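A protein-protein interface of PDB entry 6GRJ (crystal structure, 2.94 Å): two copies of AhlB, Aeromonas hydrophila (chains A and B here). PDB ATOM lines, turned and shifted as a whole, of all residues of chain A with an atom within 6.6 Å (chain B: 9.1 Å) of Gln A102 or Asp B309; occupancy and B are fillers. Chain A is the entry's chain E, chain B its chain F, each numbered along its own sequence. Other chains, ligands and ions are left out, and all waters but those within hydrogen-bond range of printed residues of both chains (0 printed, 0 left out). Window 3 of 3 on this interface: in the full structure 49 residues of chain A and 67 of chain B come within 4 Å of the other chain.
OD1 of Asp B309 is in salt-bridge range of NH1 of Arg A105 (3.0 Å). The side-chain amide nitrogen (NE2) of Gln A102 is in hydrogen-bond range of the side-chain carboxylate (OD2) of Asp B309. The side-chain amide nitrogen (NE2) of Gln A106 is in hydrogen-bond range of the backbone carbonyl oxygen (O) of Asp B309 (3.1 Å).
OG1 of Thr B316 sits at hydrogen-bond distance from O of Gln B312, at 2.8 Å. N of Thr A99 is in hydrogen-bond range of OE1 of Gln A102.
Among the printed residues, merely in contact across the chains: Val A93 with Gln B312 (3.4 Å), Arg A105 with Ile B310 (3.5 Å), Gln A106 with Ile B310 (3.5 Å), Gln A106 with Leu B313 (3.8 Å) and Val A93 with Thr B316 (3.9 Å).
Gln A102 touches one residue of chain B. Asp B309 touches just these residues of chain A: Gln A102, Arg A105 and Gln A106. No residue of chain B comes within 4 Å of Ala A101. Printed residues of chain A within 4 Å of Ile B310: Arg A105 and Gln A106. Printed residues of chain B within 4 Å of Val A93: Gln B312 and Thr B316. Printed residues of chain A within 4 Å of Gln B312: Val A93. Printed residues of chain A within 4 Å of Leu B313: Gln A106 (3.8 Å). Printed residues of chain A within 4 Å of Thr B316: Val A93. Trp B314 touches none of the printed residues of chain A. The nearest residue of chain B that does not touch Gln A102 is Ile B310 (6.4 Å). The nearest residue of chain A that does not touch Asp B309 is Val A93 (4.2 Å).
Hydrophobic or aromatic side chains of chain A within 4 Å of the printed part of chain B: Val A93. Hydrophobic or aromatic side chains of chain B that line the printed part of chain A: Ile B310 and Leu B313. Among the printed residues, 8 pairs touch across the chains. Among the printed residues, Asp or Glu carboxylates within 4 Å of a Lys or Arg side-chain nitrogen of the other chain: Arg A105 with Asp B309.
No position is printed for both chains. Of the 8 pairs that touch across the chains among the printed residues, none has its exchanged pair printed and touching as well.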
ATOM      1  N   VAL A  93     -21.650  19.096   6.545  1.00  0.00           N
ATOM      2  CA  VAL A  93     -22.988  19.572   6.794  1.00  0.00           C
ATOM      3  C   VAL A  93     -23.901  19.247   5.611  1.00  0.00           C
ATOM      4  O   VAL A  93     -25.026  18.917   5.882  1.00  0.00           O
ATOM      5  CB  VAL A  93     -23.073  21.054   7.195  1.00  0.00           C
ATOM      6  CG1 VAL A  93     -22.045  21.422   8.252  1.00  0.00           C
ATOM      7  CG2 VAL A  93     -23.010  22.000   6.008  1.00  0.00           C
ATOM      8  N   LEU A  94     -23.429  19.274   4.361  1.00  0.00           N
ATOM      9  CA  LEU A  94     -24.262  18.836   3.258  1.00  0.00           C
ATOM     10  C   LEU A  94     -24.128  17.324   3.181  1.00  0.00           C
ATOM     11  O   LEU A  94     -23.071  16.812   2.829  1.00  0.00           O
ATOM     12  CB  LEU A  94     -23.846  19.525   1.956  1.00  0.00           C
ATOM     13  CG  LEU A  94     -23.758  21.053   2.019  1.00  0.00           C
ATOM     14  CD1 LEU A  94     -23.438  21.622   0.647  1.00  0.00           C
ATOM     15  CD2 LEU A  94     -25.025  21.693   2.579  1.00  0.00           C
ATOM     16  N   PRO A  95     -25.189  16.538   3.480  1.00  0.00           N
ATOM     17  CA  PRO A  95     -25.080  15.076   3.396  1.00  0.00           C
ATOM     18  C   PRO A  95     -24.887  14.665   1.936  1.00  0.00           C
ATOM     19  O   PRO A  95     -25.148  15.457   1.024  1.00  0.00           O
ATOM     20  CB  PRO A  95     -26.423  14.607   3.982  1.00  0.00           C
ATOM     21  CG  PRO A  95     -27.383  15.728   3.676  1.00  0.00           C
ATOM     22  CD  PRO A  95     -26.563  17.000   3.773  1.00  0.00           C
ATOM     23  N   GLY A  97     -25.778  13.805  -1.625  1.00  0.00           N
ATOM     24  CA  GLY A  97     -27.007  14.090  -2.407  1.00  0.00           C
ATOM     25  C   GLY A  97     -27.831  15.213  -1.804  1.00  0.00           C
ATOM     26  O   GLY A  97     -28.772  15.049  -1.006  1.00  0.00           O
ATOM     27  N   SER A  98     -27.432  16.441  -2.161  1.00  0.00           N
ATOM     28  CA  SER A  98     -28.028  17.700  -1.622  1.00  0.00           C
ATOM     29  C   SER A  98     -28.058  18.763  -2.735  1.00  0.00           C
ATOM     30  O   SER A  98     -27.234  18.717  -3.677  1.00  0.00           O
ATOM     31  CB  SER A  98     -27.308  18.130  -0.359  1.00  0.00           C
ATOM     32  OG  SER A  98     -27.021  17.018   0.486  1.00  0.00           O
ATOM     33  N   THR A  99     -29.068  19.628  -2.695  1.00  0.00           N
ATOM     34  CA  THR A  99     -29.380  20.452  -3.869  1.00  0.00           C
ATOM     35  C   THR A  99     -28.165  21.271  -4.291  1.00  0.00           C
ATOM     36  O   THR A  99     -27.369  21.727  -3.477  1.00  0.00           O
ATOM     37  CB  THR A  99     -30.570  21.418  -3.692  1.00  0.00           C
ATOM     38  OG1 THR A  99     -30.619  21.829  -2.326  1.00  0.00           O
ATOM     39  CG2 THR A  99     -31.909  20.849  -4.111  1.00  0.00           C
ATOM     40  N   LYS A 100     -28.062  21.437  -5.614  1.00  0.00           N
ATOM     41  CA  LYS A 100     -27.093  22.290  -6.249  1.00  0.00           C
ATOM     42  C   LYS A 100     -27.293  23.698  -5.650  1.00  0.00           C
ATOM     43  O   LYS A 100     -26.353  24.452  -5.499  1.00  0.00           O
ATOM     44  CB  LYS A 100     -27.310  22.181  -7.761  1.00  0.00           C
ATOM     45  CG  LYS A 100     -26.157  22.613  -8.643  1.00  0.00           C
ATOM     46  CD  LYS A 100     -26.224  22.023 -10.041  1.00  0.00           C
ATOM     47  CE  LYS A 100     -27.343  22.549 -10.922  1.00  0.00           C
ATOM     48  NZ  LYS A 100     -27.206  23.994 -11.231  1.00  0.00           N
ATOM     49  N   ALA A 101     -28.539  24.007  -5.276  1.00  0.00           N
ATOM     50  CA  ALA A 101     -28.931  25.271  -4.677  1.00  0.00           C
ATOM     51  C   ALA A 101     -28.212  25.497  -3.339  1.00  0.00           C
ATOM     52  O   ALA A 101     -27.712  26.610  -3.098  1.00  0.00           O
ATOM     53  CB  ALA A 101     -30.431  25.295  -4.503  1.00  0.00           C
ATOM     54  N   GLN A 102     -28.174  24.457  -2.485  1.00  0.00           N
ATOM     55  CA  GLN A 102     -27.558  24.499  -1.149  1.00  0.00           C
ATOM     56  C   GLN A 102     -26.036  24.663  -1.231  1.00  0.00           C
ATOM     57  O   GLN A 102     -25.423  25.411  -0.421  1.00  0.00           O
ATOM     58  CB  GLN A 102     -27.740  23.185  -0.390  1.00  0.00           C
ATOM     59  CG  GLN A 102     -29.137  22.926   0.128  1.00  0.00           C
ATOM     60  CD  GLN A 102     -29.222  21.511   0.651  1.00  0.00           C
ATOM     61  OE1 GLN A 102     -28.837  20.554  -0.008  1.00  0.00           O
ATOM     62  NE2 GLN A 102     -29.721  21.362   1.863  1.00  0.00           N
ATOM     63  N   TRP A 103     -25.451  23.869  -2.144  1.00  0.00           N
ATOM     64  CA  TRP A 103     -24.036  23.853  -2.421  1.00  0.00           C
ATOM     65  C   TRP A 103     -23.551  25.249  -2.830  1.00  0.00           C
ATOM     66  O   TRP A 103     -22.584  25.731  -2.260  1.00  0.00           O
ATOM     67  CB  TRP A 103     -23.721  22.801  -3.493  1.00  0.00           C
ATOM     68  CG  TRP A 103     -23.247  21.503  -2.934  1.00  0.00           C
ATOM     69  CD1 TRP A 103     -23.986  20.382  -2.707  1.00  0.00           C
ATOM     70  CD2 TRP A 103     -21.919  21.211  -2.478  1.00  0.00           C
ATOM     71  NE1 TRP A 103     -23.204  19.407  -2.149  1.00  0.00           N
ATOM     72  CE2 TRP A 103     -21.932  19.886  -1.994  1.00  0.00           C
ATOM     73  CE3 TRP A 103     -20.726  21.938  -2.428  1.00  0.00           C
ATOM     74  CZ2 TRP A 103     -20.799  19.275  -1.464  1.00  0.00           C
ATOM     75  CZ3 TRP A 103     -19.601  21.329  -1.915  1.00  0.00           C
ATOM     76  CH2 TRP A 103     -19.641  20.016  -1.436  1.00  0.00           C
ATOM     77  N   LEU A 104     -24.251  25.885  -3.781  1.00  0.00           N
ATOM     78  CA  LEU A 104     -23.896  27.218  -4.250  1.00  0.00           C
ATOM     79  C   LEU A 104     -23.957  28.245  -3.110  1.00  0.00           C
ATOM     80  O   LEU A 104     -23.157  29.183  -3.120  1.00  0.00           O
ATOM     81  CB  LEU A 104     -24.826  27.645  -5.396  1.00  0.00           C
ATOM     82  CG  LEU A 104     -24.633  26.948  -6.742  1.00  0.00           C
ATOM     83  CD1 LEU A 104     -25.554  27.530  -7.807  1.00  0.00           C
ATOM     84  CD2 LEU A 104     -23.194  27.056  -7.205  1.00  0.00           C
ATOM     85  N   ARG A 105     -24.894  28.101  -2.158  1.00  0.00           N
ATOM     86  CA  ARG A 105     -24.975  29.066  -1.054  1.00  0.00           C
ATOM     87  C   ARG A 105     -23.739  28.892  -0.149  1.00  0.00           C
ATOM     88  O   ARG A 105     -23.066  29.899   0.229  1.00  0.00           O
ATOM     89  CB  ARG A 105     -26.282  28.906  -0.271  1.00  0.00           C
ATOM     90  CG  ARG A 105     -27.537  29.358  -1.011  1.00  0.00           C
ATOM     91  CD  ARG A 105     -28.856  28.784  -0.514  1.00  0.00           C
ATOM     92  NE  ARG A 105     -29.123  28.970   0.910  1.00  0.00           N
ATOM     93  CZ  ARG A 105     -28.777  28.119   1.879  1.00  0.00           C
ATOM     94  NH1 ARG A 105     -28.106  27.009   1.617  1.00  0.00           N
ATOM     95  NH2 ARG A 105     -29.120  28.372   3.131  1.00  0.00           N
ATOM     96  N   GLN A 106     -23.414  27.614   0.136  1.00  0.00           N
ATOM     97  CA  GLN A 106     -22.315  27.279   1.028  1.00  0.00           C
ATOM     98  C   GLN A 106     -20.974  27.709   0.395  1.00  0.00           C
ATOM     99  O   GLN A 106     -20.087  28.210   1.093  1.00  0.00           O
ATOM    100  CB  GLN A 106     -22.421  25.786   1.370  1.00  0.00           C
ATOM    101  CG  GLN A 106     -23.683  25.385   2.130  1.00  0.00           C
ATOM    102  CD  GLN A 106     -23.444  25.142   3.599  1.00  0.00           C
ATOM    103  OE1 GLN A 106     -22.409  24.587   3.954  1.00  0.00           O
ATOM    104  NE2 GLN A 106     -24.400  25.526   4.439  1.00  0.00           N
ATOM    105  N   LEU A 107     -20.829  27.567  -0.929  1.00  0.00           N
ATOM    106  CA  LEU A 107     -19.612  28.002  -1.590  1.00  0.00           C
ATOM    107  C   LEU A 107     -19.564  29.530  -1.593  1.00  0.00           C
ATOM    108  O   LEU A 107     -18.508  30.107  -1.332  1.00  0.00           O
ATOM    109  CB  LEU A 107     -19.547  27.488  -3.029  1.00  0.00           C
ATOM    110  CG  LEU A 107     -19.420  25.974  -3.223  1.00  0.00           C
ATOM    111  CD1 LEU A 107     -19.308  25.623  -4.695  1.00  0.00           C
ATOM    112  CD2 LEU A 107     -18.252  25.386  -2.497  1.00  0.00           C
ATOM    113  N   ALA B  92     -23.186  22.653  17.164  1.00  0.00           N
ATOM    114  CA  ALA B  92     -23.517  23.107  15.807  1.00  0.00           C
ATOM    115  C   ALA B  92     -24.962  22.776  15.433  1.00  0.00           C
ATOM    116  O   ALA B  92     -25.515  23.418  14.560  1.00  0.00           O
ATOM    117  CB  ALA B  92     -22.543  22.515  14.809  1.00  0.00           C
ATOM    118  N   LYS B 302     -21.827  34.977  12.841  1.00  0.00           N
ATOM    119  CA  LYS B 302     -22.390  34.635  11.534  1.00  0.00           C
ATOM    120  C   LYS B 302     -23.256  33.374  11.613  1.00  0.00           C
ATOM    121  O   LYS B 302     -24.091  33.158  10.743  1.00  0.00           O
ATOM    122  CB  LYS B 302     -21.289  34.520  10.479  1.00  0.00           C
ATOM    123  CG  LYS B 302     -20.757  35.869  10.004  1.00  0.00           C
ATOM    124  CD  LYS B 302     -19.904  35.789   8.769  1.00  0.00           C
ATOM    125  CE  LYS B 302     -19.178  37.077   8.463  1.00  0.00           C
ATOM    126  NZ  LYS B 302     -20.131  38.036   7.865  1.00  0.00           N
ATOM    127  N   GLY B 303     -23.108  32.580  12.674  1.00  0.00           N
ATOM    128  CA  GLY B 303     -23.928  31.378  12.869  1.00  0.00           C
ATOM    129  C   GLY B 303     -25.247  31.669  13.573  1.00  0.00           C
ATOM    130  O   GLY B 303     -26.229  30.938  13.437  1.00  0.00           O
ATOM    131  N   SER B 306     -27.859  33.393  10.708  1.00  0.00           N
ATOM    132  CA  SER B 306     -27.830  32.696   9.413  1.00  0.00           C
ATOM    133  C   SER B 306     -28.878  31.578   9.318  1.00  0.00           C
ATOM    134  O   SER B 306     -29.374  31.122  10.334  1.00  0.00           O
ATOM    135  CB  SER B 306     -26.442  32.160   9.156  1.00  0.00           C
ATOM    136  OG  SER B 306     -26.064  31.247  10.176  1.00  0.00           O
ATOM    137  N   GLY B 307     -29.156  31.167   8.058  1.00  0.00           N
ATOM    138  CA  GLY B 307     -30.112  30.093   7.606  1.00  0.00           C
ATOM    139  C   GLY B 307     -29.919  28.772   8.331  1.00  0.00           C
ATOM    140  O   GLY B 307     -29.189  28.765   9.273  1.00  0.00           O
ATOM    141  N   ASP B 308     -30.626  27.701   7.954  1.00  0.00           N
ATOM    142  CA  ASP B 308     -30.619  26.498   8.779  1.00  0.00           C
ATOM    143  C   ASP B 308     -29.322  25.712   8.569  1.00  0.00           C
ATOM    144  O   ASP B 308     -28.685  25.332   9.558  1.00  0.00           O
ATOM    145  CB  ASP B 308     -31.902  25.676   8.609  1.00  0.00           C
ATOM    146  CG  ASP B 308     -33.090  26.263   9.354  1.00  0.00           C
ATOM    147  OD1 ASP B 308     -32.913  26.647  10.527  1.00  0.00           O
ATOM    148  OD2 ASP B 308     -34.174  26.345   8.756  1.00  0.00           O
ATOM    149  N   ASP B 309     -28.910  25.500   7.312  1.00  0.00           N
ATOM    150  CA  ASP B 309     -27.663  24.727   7.075  1.00  0.00           C
ATOM    151  C   ASP B 309     -26.449  25.684   7.075  1.00  0.00           C
ATOM    152  O   ASP B 309     -25.348  25.241   7.390  1.00  0.00           O
ATOM    153  CB  ASP B 309     -27.782  23.752   5.890  1.00  0.00           C
ATOM    154  CG  ASP B 309     -28.072  24.339   4.515  1.00  0.00           C
ATOM    155  OD1 ASP B 309     -27.650  25.491   4.222  1.00  0.00           O
ATOM    156  OD2 ASP B 309     -28.683  23.618   3.732  1.00  0.00           O
ATOM    157  N   ILE B 310     -26.640  26.981   6.766  1.00  0.00           N
ATOM    158  CA  ILE B 310     -25.540  27.983   6.837  1.00  0.00           C
ATOM    159  C   ILE B 310     -25.122  28.154   8.308  1.00  0.00           C
ATOM    160  O   ILE B 310     -23.943  28.367   8.621  1.00  0.00           O
ATOM    161  CB  ILE B 310     -25.922  29.340   6.211  1.00  0.00           C
ATOM    162  CG1 ILE B 310     -26.096  29.224   4.692  1.00  0.00           C
ATOM    163  CG2 ILE B 310     -24.900  30.419   6.568  1.00  0.00           C
ATOM    164  CD1 ILE B 310     -26.384  30.540   3.978  1.00  0.00           C
ATOM    165  N   ARG B 311     -26.114  28.084   9.200  1.00  0.00           N
ATOM    166  CA  ARG B 311     -25.906  28.161  10.636  1.00  0.00           C
ATOM    167  C   ARG B 311     -24.993  27.016  11.075  1.00  0.00           C
ATOM    168  O   ARG B 311     -24.050  27.215  11.842  1.00  0.00           O
ATOM    169  CB  ARG B 311     -27.249  28.090  11.367  1.00  0.00           C
ATOM    170  CG  ARG B 311     -27.165  27.886  12.870  1.00  0.00           C
ATOM    171  CD  ARG B 311     -28.448  28.250  13.571  1.00  0.00           C
ATOM    172  NE  ARG B 311     -28.685  29.667  13.354  1.00  0.00           N
ATOM    173  CZ  ARG B 311     -29.737  30.324  13.787  1.00  0.00           C
ATOM    174  NH1 ARG B 311     -30.655  29.707  14.507  1.00  0.00           N
ATOM    175  NH2 ARG B 311     -29.875  31.598  13.474  1.00  0.00           N
ATOM    176  N   GLN B 312     -25.283  25.818  10.558  1.00  0.00           N
ATOM    177  CA  GLN B 312     -24.524  24.656  10.920  1.00  0.00           C
ATOM    178  C   GLN B 312     -23.088  24.801  10.395  1.00  0.00           C
ATOM    179  O   GLN B 312     -22.152  24.425  11.088  1.00  0.00           O
ATOM    180  CB  GLN B 312     -25.238  23.398  10.439  1.00  0.00           C
ATOM    181  CG  GLN B 312     -24.664  22.137  11.034  1.00  0.00           C
ATOM    182  CD  GLN B 312     -25.146  20.915  10.303  1.00  0.00           C
ATOM    183  OE1 GLN B 312     -25.738  20.987   9.227  1.00  0.00           O
ATOM    184  NE2 GLN B 312     -24.887  19.760  10.890  1.00  0.00           N
ATOM    185  N   LEU B 313     -22.910  25.362   9.197  1.00  0.00           N
ATOM    186  CA  LEU B 313     -21.576  25.566   8.641  1.00  0.00           C
ATOM    187  C   LEU B 313     -20.733  26.392   9.619  1.00  0.00           C
ATOM    188  O   LEU B 313     -19.661  25.943  10.048  1.00  0.00           O
ATOM    189  CB  LEU B 313     -21.662  26.280   7.284  1.00  0.00           C
ATOM    190  CG  LEU B 313     -20.322  26.723   6.691  1.00  0.00           C
ATOM    191  CD1 LEU B 313     -19.429  25.512   6.413  1.00  0.00           C
ATOM    192  CD2 LEU B 313     -20.527  27.586   5.454  1.00  0.00           C
ATOM    193  N   TRP B 314     -21.237  27.583   9.971  1.00  0.00           N
ATOM    194  CA  TRP B 314     -20.513  28.511  10.815  1.00  0.00           C
ATOM    195  C   TRP B 314     -20.240  27.943  12.218  1.00  0.00           C
ATOM    196  O   TRP B 314     -19.175  28.189  12.801  1.00  0.00           O
ATOM    197  CB  TRP B 314     -21.252  29.838  10.907  1.00  0.00           C
ATOM    198  CG  TRP B 314     -21.146  30.680   9.688  1.00  0.00           C
ATOM    199  CD1 TRP B 314     -22.153  30.932   8.803  1.00  0.00           C
ATOM    200  CD2 TRP B 314     -20.019  31.423   9.219  1.00  0.00           C
ATOM    201  NE1 TRP B 314     -21.726  31.768   7.809  1.00  0.00           N
ATOM    202  CE2 TRP B 314     -20.416  32.079   8.035  1.00  0.00           C
ATOM    203  CE3 TRP B 314     -18.707  31.575   9.667  1.00  0.00           C
ATOM    204  CZ2 TRP B 314     -19.551  32.875   7.294  1.00  0.00           C
ATOM    205  CZ3 TRP B 314     -17.854  32.374   8.937  1.00  0.00           C
ATOM    206  CH2 TRP B 314     -18.270  33.013   7.771  1.00  0.00           C
ATOM    207  N   LEU B 315     -21.202  27.202  12.770  1.00  0.00           N
ATOM    208  CA  LEU B 315     -21.033  26.667  14.098  1.00  0.00           C
ATOM    209  C   LEU B 315     -20.031  25.508  14.076  1.00  0.00           C
ATOM    210  O   LEU B 315     -19.289  25.330  15.035  1.00  0.00           O
ATOM    211  CB  LEU B 315     -22.394  26.257  14.664  1.00  0.00           C
ATOM    212  CG  LEU B 315     -23.360  27.425  14.895  1.00  0.00           C
ATOM    213  CD1 LEU B 315     -24.617  26.927  15.561  1.00  0.00           C
ATOM    214  CD2 LEU B 315     -22.745  28.568  15.702  1.00  0.00           C
ATOM    215  N   THR B 316     -19.997  24.735  12.987  1.00  0.00           N
ATOM    216  CA  THR B 316     -19.001  23.656  12.822  1.00  0.00           C
ATOM    217  C   THR B 316     -17.606  24.289  12.774  1.00  0.00           C
ATOM    218  O   THR B 316     -16.675  23.802  13.416  1.00  0.00           O
ATOM    219  CB  THR B 316     -19.292  22.795  11.589  1.00  0.00           C
ATOM    220  OG1 THR B 316     -20.593  22.243  11.750  1.00  0.00           O
ATOM    221  CG2 THR B 316     -18.321  21.645  11.433  1.00  0.00           C
